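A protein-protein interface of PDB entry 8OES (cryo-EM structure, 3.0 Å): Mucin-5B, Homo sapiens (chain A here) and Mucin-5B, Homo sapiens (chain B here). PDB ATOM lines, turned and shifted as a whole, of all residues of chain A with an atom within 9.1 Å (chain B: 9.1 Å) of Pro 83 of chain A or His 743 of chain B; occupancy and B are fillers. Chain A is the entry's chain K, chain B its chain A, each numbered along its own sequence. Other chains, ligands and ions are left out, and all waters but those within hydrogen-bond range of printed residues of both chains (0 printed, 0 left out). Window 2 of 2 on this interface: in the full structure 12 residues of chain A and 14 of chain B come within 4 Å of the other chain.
Of chain B, only His 743 comes within 4 Å of Pro 83 of chain A. His 743 of chain B touches just these residues of chain A: Pro 82, Pro 83 and Leu 84. No residue of chain B comes within 4 Å of Gly 20 of chain A. No residue of chain A comes within 4 Å of Gly 746 of chain B. Of the printed residues of chain B, Pro 82 of chain A touches His 743. Printed residues of chain A within 4 Å of Val 742 of chain B: Leu 84. Of the printed residues of chain B, Cys 85 of chain A touches Glu 740 (3.6 Å). The nearest residue of chain B that does not touch Pro 83 of chain A is Asp 744 of chain B (5.6 Å). The nearest residue of chain A that does not touch His 743 of chain B is Ser 81 of chain A (5.9 Å).
The backbone carbonyl oxygen (O) of Val 742 of chain B sits at hydrogen-bond distance from the backbone NH (N) of Cys 749 of chain B (2.9 Å). O of Ala 747 of chain B lies within hydrogen-bond range of ND1 of His 743 of chain B (2.8 Å). SG of Cys 75 of chain A forms a disulfide with SG of Cys 85 of chain A (2.0 Å). The backbone NH (N) of Ala 76 of chain A sits at hydrogen-bond distance from the side-chain sulfur (SG) of Cys 85 of chain A. N of Cys 85 of chain A is in hydrogen-bond range of OD1 of Asn 77 of chain A, 3.3 Å away. The side-chain sulfur (SG) of Cys 749 of chain B forms a disulfide with the side-chain sulfur (SG) of Cys 758 of chain B.
Of the 17 printed residues of chain B, 4 touch a printed residue of chain A. Among the printed residues, 7 pairs touch across the chains. Among the printed residues, no Asp or Glu carboxylate lies within 4 Å of a Lys or Arg side-chain nitrogen of the other chain.
Among the printed residues, merely in contact across the chains: Pro 82 of chain A with His 743 of chain B (2.8 Å), Pro 83 of chain A with His 743 of chain B (3.7 Å), Leu 84 of chain A with Val 741 of chain B (2.9 Å), Leu 84 of chain A with Val 742 of chain B (3.4 Å), Leu 84 of chain A with His 743 of chain B (3.6 Å), Cys 85 of chain A with Glu 740 of chain B (3.6 Å) and His 86 of chain A with Glu 740 of chain B (3.3 Å).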
ATOM      1  N   PRO A  17      17.183  10.072 -24.112  1.00  0.00           N
ATOM      2  CA  PRO A  17      17.868   8.885 -23.587  1.00  0.00           C
ATOM      3  C   PRO A  17      17.331   7.598 -24.193  1.00  0.00           C
ATOM      4  O   PRO A  17      16.141   7.469 -24.489  1.00  0.00           O
ATOM      5  CB  PRO A  17      17.601   8.959 -22.078  1.00  0.00           C
ATOM      6  CG  PRO A  17      16.494   9.938 -21.924  1.00  0.00           C
ATOM      7  CD  PRO A  17      16.634  10.910 -23.037  1.00  0.00           C
ATOM      8  N   GLU A  18      18.227   6.652 -24.384  1.00  0.00           N
ATOM      9  CA  GLU A  18      17.994   5.424 -25.125  1.00  0.00           C
ATOM     10  C   GLU A  18      17.733   4.269 -24.175  1.00  0.00           C
ATOM     11  O   GLU A  18      18.440   4.135 -23.165  1.00  0.00           O
ATOM     12  CB  GLU A  18      19.206   5.110 -25.997  1.00  0.00           C
ATOM     13  CG  GLU A  18      19.641   6.268 -26.881  1.00  0.00           C
ATOM     14  CD  GLU A  18      21.042   6.081 -27.427  1.00  0.00           C
ATOM     15  OE1 GLU A  18      21.711   5.106 -27.025  1.00  0.00           O
ATOM     16  OE2 GLU A  18      21.477   6.909 -28.254  1.00  0.00           O
ATOM     17  N   PRO A  19      16.741   3.427 -24.450  1.00  0.00           N
ATOM     18  CA  PRO A  19      16.541   2.232 -23.626  1.00  0.00           C
ATOM     19  C   PRO A  19      17.685   1.248 -23.802  1.00  0.00           C
ATOM     20  O   PRO A  19      18.305   1.162 -24.865  1.00  0.00           O
ATOM     21  CB  PRO A  19      15.222   1.656 -24.147  1.00  0.00           C
ATOM     22  CG  PRO A  19      15.138   2.137 -25.551  1.00  0.00           C
ATOM     23  CD  PRO A  19      15.803   3.485 -25.584  1.00  0.00           C
ATOM     24  N   GLY A  20      17.962   0.494 -22.734  1.00  0.00           N
ATOM     25  CA  GLY A  20      19.027  -0.483 -22.721  1.00  0.00           C
ATOM     26  C   GLY A  20      19.880  -0.317 -21.484  1.00  0.00           C
ATOM     27  O   GLY A  20      19.440   0.240 -20.472  1.00  0.00           O
ATOM     28  N   LEU A  21      21.116  -0.807 -21.569  1.00  0.00           N
ATOM     29  CA  LEU A  21      22.062  -0.727 -20.463  1.00  0.00           C
ATOM     30  C   LEU A  21      23.073   0.400 -20.620  1.00  0.00           C
ATOM     31  O   LEU A  21      23.357   1.111 -19.651  1.00  0.00           O
ATOM     32  CB  LEU A  21      22.808  -2.052 -20.303  1.00  0.00           C
ATOM     33  CG  LEU A  21      22.056  -3.127 -19.524  1.00  0.00           C
ATOM     34  CD1 LEU A  21      22.859  -4.411 -19.498  1.00  0.00           C
ATOM     35  CD2 LEU A  21      21.748  -2.646 -18.117  1.00  0.00           C
ATOM     36  N   GLY A  22      23.633   0.579 -21.814  1.00  0.00           N
ATOM     37  CA  GLY A  22      24.546   1.681 -22.032  1.00  0.00           C
ATOM     38  C   GLY A  22      23.884   3.007 -22.308  1.00  0.00           C
ATOM     39  O   GLY A  22      24.575   4.028 -22.378  1.00  0.00           O
ATOM     40  N   GLY A  23      22.562   3.019 -22.454  1.00  0.00           N
ATOM     41  CA  GLY A  23      21.845   4.222 -22.808  1.00  0.00           C
ATOM     42  C   GLY A  23      21.778   5.219 -21.671  1.00  0.00           C
ATOM     43  O   GLY A  23      22.339   5.033 -20.593  1.00  0.00           O
ATOM     44  N   GLY A  24      21.073   6.307 -21.932  1.00  0.00           N
ATOM     45  CA  GLY A  24      20.895   7.368 -20.973  1.00  0.00           C
ATOM     46  C   GLY A  24      21.048   8.710 -21.644  1.00  0.00           C
ATOM     47  O   GLY A  24      21.087   8.815 -22.867  1.00  0.00           O
ATOM     48  N   CYS A  75      23.147  11.016 -16.948  1.00  0.00           N
ATOM     49  CA  CYS A  75      22.334   9.948 -16.377  1.00  0.00           C
ATOM     50  C   CYS A  75      22.612   8.690 -17.181  1.00  0.00           C
ATOM     51  O   CYS A  75      22.385   8.674 -18.396  1.00  0.00           O
ATOM     52  CB  CYS A  75      20.841  10.285 -16.436  1.00  0.00           C
ATOM     53  SG  CYS A  75      19.737   9.080 -15.640  1.00  0.00           S
ATOM     54  N   ALA A  76      23.091   7.645 -16.515  1.00  0.00           N
ATOM     55  CA  ALA A  76      23.419   6.378 -17.153  1.00  0.00           C
ATOM     56  C   ALA A  76      22.365   5.336 -16.814  1.00  0.00           C
ATOM     57  O   ALA A  76      21.907   5.253 -15.671  1.00  0.00           O
ATOM     58  CB  ALA A  76      24.798   5.882 -16.716  1.00  0.00           C
ATOM     59  N   ASN A  77      21.984   4.542 -17.814  1.00  0.00           N
ATOM     60  CA  ASN A  77      20.917   3.568 -17.614  1.00  0.00           C
ATOM     61  C   ASN A  77      21.295   2.521 -16.577  1.00  0.00           C
ATOM     62  O   ASN A  77      20.487   2.180 -15.707  1.00  0.00           O
ATOM     63  CB  ASN A  77      20.568   2.894 -18.938  1.00  0.00           C
ATOM     64  CG  ASN A  77      19.654   3.736 -19.790  1.00  0.00           C
ATOM     65  OD1 ASN A  77      19.433   4.909 -19.500  1.00  0.00           O
ATOM     66  ND2 ASN A  77      19.122   3.145 -20.854  1.00  0.00           N
ATOM     67  N   SER A  78      22.525   2.008 -16.642  1.00  0.00           N
ATOM     68  CA  SER A  78      22.886   0.848 -15.834  1.00  0.00           C
ATOM     69  C   SER A  78      22.893   1.142 -14.339  1.00  0.00           C
ATOM     70  O   SER A  78      22.806   0.203 -13.541  1.00  0.00           O
ATOM     71  CB  SER A  78      24.254   0.320 -16.268  1.00  0.00           C
ATOM     72  OG  SER A  78      25.304   1.020 -15.624  1.00  0.00           O
ATOM     73  N   GLN A  79      22.975   2.407 -13.936  1.00  0.00           N
ATOM     74  CA  GLN A  79      23.110   2.743 -12.525  1.00  0.00           C
ATOM     75  C   GLN A  79      21.783   2.795 -11.776  1.00  0.00           C
ATOM     76  O   GLN A  79      21.795   2.860 -10.543  1.00  0.00           O
ATOM     77  CB  GLN A  79      23.839   4.081 -12.372  1.00  0.00           C
ATOM     78  CG  GLN A  79      25.309   4.029 -12.758  1.00  0.00           C
ATOM     79  CD  GLN A  79      25.979   5.387 -12.692  1.00  0.00           C
ATOM     80  OE1 GLN A  79      25.312   6.419 -12.636  1.00  0.00           O
ATOM     81  NE2 GLN A  79      27.306   5.393 -12.707  1.00  0.00           N
ATOM     82  N   GLN A  80      20.651   2.763 -12.471  1.00  0.00           N
ATOM     83  CA  GLN A  80      19.345   2.859 -11.839  1.00  0.00           C
ATOM     84  C   GLN A  80      18.606   1.538 -11.974  1.00  0.00           C
ATOM     85  O   GLN A  80      18.953   0.691 -12.799  1.00  0.00           O
ATOM     86  CB  GLN A  80      18.507   3.981 -12.458  1.00  0.00           C
ATOM     87  CG  GLN A  80      19.305   4.984 -13.272  1.00  0.00           C
ATOM     88  CD  GLN A  80      20.102   5.933 -12.408  1.00  0.00           C
ATOM     89  OE1 GLN A  80      19.715   6.240 -11.281  1.00  0.00           O
ATOM     90  NE2 GLN A  80      21.224   6.411 -12.933  1.00  0.00           N
ATOM     91  N   SER A  81      17.578   1.367 -11.145  1.00  0.00           N
ATOM     92  CA  SER A  81      16.683   0.218 -11.243  1.00  0.00           C
ATOM     93  C   SER A  81      15.254   0.733 -11.338  1.00  0.00           C
ATOM     94  O   SER A  81      14.793   1.439 -10.416  1.00  0.00           O
ATOM     95  CB  SER A  81      16.836  -0.732 -10.058  1.00  0.00           C
ATOM     96  OG  SER A  81      15.807  -1.704 -10.070  1.00  0.00           O
ATOM     97  N   PRO A  82      14.516   0.426 -12.411  1.00  0.00           N
ATOM     98  CA  PRO A  82      14.909  -0.274 -13.645  1.00  0.00           C
ATOM     99  C   PRO A  82      16.064   0.409 -14.366  1.00  0.00           C
ATOM    100  O   PRO A  82      16.255   1.615 -14.235  1.00  0.00           O
ATOM    101  CB  PRO A  82      13.602  -0.227 -14.482  1.00  0.00           C
ATOM    102  CG  PRO A  82      12.668   0.689 -13.676  1.00  0.00           C
ATOM    103  CD  PRO A  82      13.061   0.336 -12.302  1.00  0.00           C
ATOM    104  N   PRO A  83      16.856  -0.334 -15.130  1.00  0.00           N
ATOM    105  CA  PRO A  83      18.043   0.264 -15.753  1.00  0.00           C
ATOM    106  C   PRO A  83      17.692   1.244 -16.856  1.00  0.00           C
ATOM    107  O   PRO A  83      17.937   0.977 -18.034  1.00  0.00           O
ATOM    108  CB  PRO A  83      18.798  -0.951 -16.302  1.00  0.00           C
ATOM    109  CG  PRO A  83      17.729  -1.966 -16.545  1.00  0.00           C
ATOM    110  CD  PRO A  83      16.716  -1.762 -15.457  1.00  0.00           C
ATOM    111  N   LEU A  84      17.117   2.384 -16.483  1.00  0.00           N
ATOM    112  CA  LEU A  84      16.707   3.386 -17.452  1.00  0.00           C
ATOM    113  C   LEU A  84      16.904   4.771 -16.858  1.00  0.00           C
ATOM    114  O   LEU A  84      17.192   4.927 -15.670  1.00  0.00           O
ATOM    115  CB  LEU A  84      15.250   3.185 -17.882  1.00  0.00           C
ATOM    116  CG  LEU A  84      15.015   2.106 -18.938  1.00  0.00           C
ATOM    117  CD1 LEU A  84      14.677   0.774 -18.296  1.00  0.00           C
ATOM    118  CD2 LEU A  84      13.928   2.540 -19.903  1.00  0.00           C
ATOM    119  N   CYS A  85      16.749   5.777 -17.707  1.00  0.00           N
ATOM    120  CA  CYS A  85      16.812   7.174 -17.314  1.00  0.00           C
ATOM    121  C   CYS A  85      15.576   7.902 -17.818  1.00  0.00           C
ATOM    122  O   CYS A  85      14.853   7.422 -18.695  1.00  0.00           O
ATOM    123  CB  CYS A  85      18.074   7.857 -17.860  1.00  0.00           C
ATOM    124  SG  CYS A  85      19.591   7.531 -16.949  1.00  0.00           S
ATOM    125  N   HIS A  86      15.334   9.073 -17.241  1.00  0.00           N
ATOM    126  CA  HIS A  86      14.318   9.976 -17.749  1.00  0.00           C
ATOM    127  C   HIS A  86      14.958  10.906 -18.776  1.00  0.00           C
ATOM    128  O   HIS A  86      16.170  10.891 -18.989  1.00  0.00           O
ATOM    129  CB  HIS A  86      13.677  10.748 -16.600  1.00  0.00           C
ATOM    130  CG  HIS A  86      13.103   9.870 -15.532  1.00  0.00           C
ATOM    131  ND1 HIS A  86      13.380  10.048 -14.194  1.00  0.00           N
ATOM    132  CD2 HIS A  86      12.274   8.802 -15.606  1.00  0.00           C
ATOM    133  CE1 HIS A  86      12.739   9.132 -13.489  1.00  0.00           C
ATOM    134  NE2 HIS A  86      12.060   8.364 -14.322  1.00  0.00           N
ATOM    135  N   ALA B 731       6.413   3.038  -9.122  1.00  0.00           N
ATOM    136  CA  ALA B 731       6.598   1.632  -8.788  1.00  0.00           C
ATOM    137  C   ALA B 731       7.650   1.515  -7.697  1.00  0.00           C
ATOM    138  O   ALA B 731       8.766   2.020  -7.853  1.00  0.00           O
ATOM    139  CB  ALA B 731       7.014   0.821 -10.017  1.00  0.00           C
ATOM    140  N   LEU B 736       8.639   6.876 -12.055  1.00  0.00           N
ATOM    141  CA  LEU B 736       8.765   6.265 -13.372  1.00  0.00           C
ATOM    142  C   LEU B 736       8.022   7.170 -14.341  1.00  0.00           C
ATOM    143  O   LEU B 736       6.788   7.213 -14.333  1.00  0.00           O
ATOM    144  CB  LEU B 736       8.203   4.845 -13.375  1.00  0.00           C
ATOM    145  CG  LEU B 736       8.517   3.969 -14.586  1.00  0.00           C
ATOM    146  CD1 LEU B 736       7.590   4.217 -15.762  1.00  0.00           C
ATOM    147  CD2 LEU B 736       9.964   4.171 -14.969  1.00  0.00           C
ATOM    148  N   GLU B 740       6.988   6.075 -20.674  1.00  0.00           N
ATOM    149  CA  GLU B 740       8.330   5.516 -20.621  1.00  0.00           C
ATOM    150  C   GLU B 740       8.242   4.009 -20.454  1.00  0.00           C
ATOM    151  O   GLU B 740       7.643   3.518 -19.491  1.00  0.00           O
ATOM    152  CB  GLU B 740       9.134   6.143 -19.481  1.00  0.00           C
ATOM    153  CG  GLU B 740      10.250   5.277 -18.943  1.00  0.00           C
ATOM    154  CD  GLU B 740      10.872   5.860 -17.693  1.00  0.00           C
ATOM    155  OE1 GLU B 740      10.194   6.651 -17.008  1.00  0.00           O
ATOM    156  OE2 GLU B 740      12.035   5.526 -17.387  1.00  0.00           O
ATOM    157  N   VAL B 741       8.838   3.282 -21.394  1.00  0.00           N
ATOM    158  CA  VAL B 741       8.888   1.827 -21.364  1.00  0.00           C
ATOM    159  C   VAL B 741      10.151   1.419 -20.622  1.00  0.00           C
ATOM    160  O   VAL B 741      11.243   1.924 -20.915  1.00  0.00           O
ATOM    161  CB  VAL B 741       8.863   1.243 -22.789  1.00  0.00           C
ATOM    162  CG1 VAL B 741       9.154  -0.248 -22.767  1.00  0.00           C
ATOM    163  CG2 VAL B 741       7.523   1.517 -23.448  1.00  0.00           C
ATOM    164  N   VAL B 742      10.007   0.517 -19.651  1.00  0.00           N
ATOM    165  CA  VAL B 742      11.113   0.119 -18.795  1.00  0.00           C
ATOM    166  C   VAL B 742      11.126  -1.392 -18.642  1.00  0.00           C
ATOM    167  O   VAL B 742      10.164  -2.087 -18.976  1.00  0.00           O
ATOM    168  CB  VAL B 742      11.041   0.783 -17.409  1.00  0.00           C
ATOM    169  CG1 VAL B 742      11.537   2.213 -17.492  1.00  0.00           C
ATOM    170  CG2 VAL B 742       9.618   0.722 -16.873  1.00  0.00           C
ATOM    171  N   HIS B 743      12.240  -1.890 -18.121  1.00  0.00           N
ATOM    172  CA  HIS B 743      12.431  -3.305 -17.841  1.00  0.00           C
ATOM    173  C   HIS B 743      12.507  -3.501 -16.335  1.00  0.00           C
ATOM    174  O   HIS B 743      13.133  -2.700 -15.634  1.00  0.00           O
ATOM    175  CB  HIS B 743      13.707  -3.823 -18.508  1.00  0.00           C
ATOM    176  CG  HIS B 743      13.840  -5.313 -18.486  1.00  0.00           C
ATOM    177  ND1 HIS B 743      12.886  -6.141 -17.936  1.00  0.00           N
ATOM    178  CD2 HIS B 743      14.826  -6.125 -18.936  1.00  0.00           C
ATOM    179  CE1 HIS B 743      13.274  -7.397 -18.052  1.00  0.00           C
ATOM    180  NE2 HIS B 743      14.449  -7.415 -18.656  1.00  0.00           N
ATOM    181  N   ASP B 744      11.864  -4.554 -15.840  1.00  0.00           N
ATOM    182  CA  ASP B 744      11.926  -4.870 -14.417  1.00  0.00           C
ATOM    183  C   ASP B 744      11.565  -6.331 -14.215  1.00  0.00           C
ATOM    184  O   ASP B 744      10.462  -6.750 -14.582  1.00  0.00           O
ATOM    185  CB  ASP B 744      10.988  -3.963 -13.620  1.00  0.00           C
ATOM    186  CG  ASP B 744      11.074  -4.202 -12.127  1.00  0.00           C
ATOM    187  OD1 ASP B 744      12.190  -4.454 -11.630  1.00  0.00           O
ATOM    188  OD2 ASP B 744      10.027  -4.125 -11.450  1.00  0.00           O
ATOM    189  N   GLU B 745      12.496  -7.100 -13.644  1.00  0.00           N
ATOM    190  CA  GLU B 745      12.236  -8.471 -13.195  1.00  0.00           C
ATOM    191  C   GLU B 745      11.717  -9.357 -14.324  1.00  0.00           C
ATOM    192  O   GLU B 745      10.740 -10.092 -14.161  1.00  0.00           O
ATOM    193  CB  GLU B 745      11.264  -8.476 -12.016  1.00  0.00           C
ATOM    194  CG  GLU B 745      11.490  -9.580 -11.010  1.00  0.00           C
ATOM    195  CD  GLU B 745      10.993  -9.189  -9.642  1.00  0.00           C
ATOM    196  OE1 GLU B 745      10.523  -8.041  -9.502  1.00  0.00           O
ATOM    197  OE2 GLU B 745      11.062 -10.021  -8.713  1.00  0.00           O
ATOM    198  N   GLY B 746      12.375  -9.294 -15.479  1.00  0.00           N
ATOM    199  CA  GLY B 746      11.926 -10.065 -16.621  1.00  0.00           C
ATOM    200  C   GLY B 746      10.617  -9.600 -17.216  1.00  0.00           C
ATOM    201  O   GLY B 746       9.929 -10.391 -17.865  1.00  0.00           O
ATOM    202  N   ALA B 747      10.253  -8.335 -17.016  1.00  0.00           N
ATOM    203  CA  ALA B 747       8.977  -7.805 -17.469  1.00  0.00           C
ATOM    204  C   ALA B 747       9.184  -6.454 -18.135  1.00  0.00           C
ATOM    205  O   ALA B 747      10.152  -5.745 -17.849  1.00  0.00           O
ATOM    206  CB  ALA B 747       7.986  -7.662 -16.307  1.00  0.00           C
ATOM    207  N   VAL B 748       8.256  -6.099 -19.020  1.00  0.00           N
ATOM    208  CA  VAL B 748       8.290  -4.831 -19.740  1.00  0.00           C
ATOM    209  C   VAL B 748       7.098  -3.999 -19.296  1.00  0.00           C
ATOM    210  O   VAL B 748       5.956  -4.465 -19.349  1.00  0.00           O
ATOM    211  CB  VAL B 748       8.279  -5.049 -21.263  1.00  0.00           C
ATOM    212  CG1 VAL B 748       7.726  -3.827 -21.975  1.00  0.00           C
ATOM    213  CG2 VAL B 748       9.679  -5.368 -21.754  1.00  0.00           C
ATOM    214  N   CYS B 749       7.356  -2.772 -18.860  1.00  0.00           N
ATOM    215  CA  CYS B 749       6.314  -1.930 -18.296  1.00  0.00           C
ATOM    216  C   CYS B 749       6.237  -0.607 -19.047  1.00  0.00           C
ATOM    217  O   CYS B 749       7.192  -0.170 -19.694  1.00  0.00           O
ATOM    218  CB  CYS B 749       6.545  -1.681 -16.794  1.00  0.00           C
ATOM    219  SG  CYS B 749       6.636  -3.194 -15.783  1.00  0.00           S
ATOM    220  N   SER B 750       5.065   0.014 -18.956  1.00  0.00           N
ATOM    221  CA  SER B 750       4.789   1.290 -19.594  1.00  0.00           C
ATOM    222  C   SER B 750       4.031   2.187 -18.628  1.00  0.00           C
ATOM    223  O   SER B 750       3.343   1.713 -17.716  1.00  0.00           O
ATOM    224  CB  SER B 750       3.983   1.118 -20.889  1.00  0.00           C
ATOM    225  OG  SER B 750       3.822   2.356 -21.559  1.00  0.00           O
ATOM    226  N   SER B 757       1.451  -0.059 -16.313  1.00  0.00           N
ATOM    227  CA  SER B 757       1.083  -1.351 -16.880  1.00  0.00           C
ATOM    228  C   SER B 757       2.341  -2.191 -17.016  1.00  0.00           C
ATOM    229  O   SER B 757       3.405  -1.658 -17.338  1.00  0.00           O
ATOM    230  CB  SER B 757       0.408  -1.179 -18.245  1.00  0.00           C
ATOM    231  OG  SER B 757      -0.508  -0.097 -18.236  1.00  0.00           O
ATOM    232  N   CYS B 758       2.231  -3.496 -16.771  1.00  0.00           N
ATOM    233  CA  CYS B 758       3.380  -4.388 -16.861  1.00  0.00           C
ATOM    234  C   CYS B 758       2.997  -5.688 -17.556  1.00  0.00           C
ATOM    235  O   CYS B 758       1.903  -6.222 -17.345  1.00  0.00           O
ATOM    236  CB  CYS B 758       3.972  -4.672 -15.472  1.00  0.00           C
ATOM    237  SG  CYS B 758       4.878  -3.264 -14.757  1.00  0.00           S
ATOM    238  N   LEU B 759       3.918  -6.198 -18.375  1.00  0.00           N
ATOM    239  CA  LEU B 759       3.682  -7.326 -19.261  1.00  0.00           C
ATOM    240  C   LEU B 759       4.822  -8.323 -19.137  1.00  0.00           C
ATOM    241  O   LEU B 759       5.975  -7.946 -18.895  1.00  0.00           O
ATOM    242  CB  LEU B 759       3.579  -6.873 -20.724  1.00  0.00           C
ATOM    243  CG  LEU B 759       2.724  -5.647 -21.035  1.00  0.00           C
ATOM    244  CD1 LEU B 759       3.242  -4.967 -22.284  1.00  0.00           C
ATOM    245  CD2 LEU B 759       1.272  -6.043 -21.207  1.00  0.00           C
ATOM    246  N   GLY B 760       4.494  -9.596 -19.332  1.00  0.00           N
ATOM    247  CA  GLY B 760       5.482 -10.659 -19.282  1.00  0.00           C
ATOM    248  C   GLY B 760       5.545 -11.381 -17.950  1.00  0.00           C
ATOM    249  O   GLY B 760       6.393 -12.248 -17.744  1.00  0.00           O
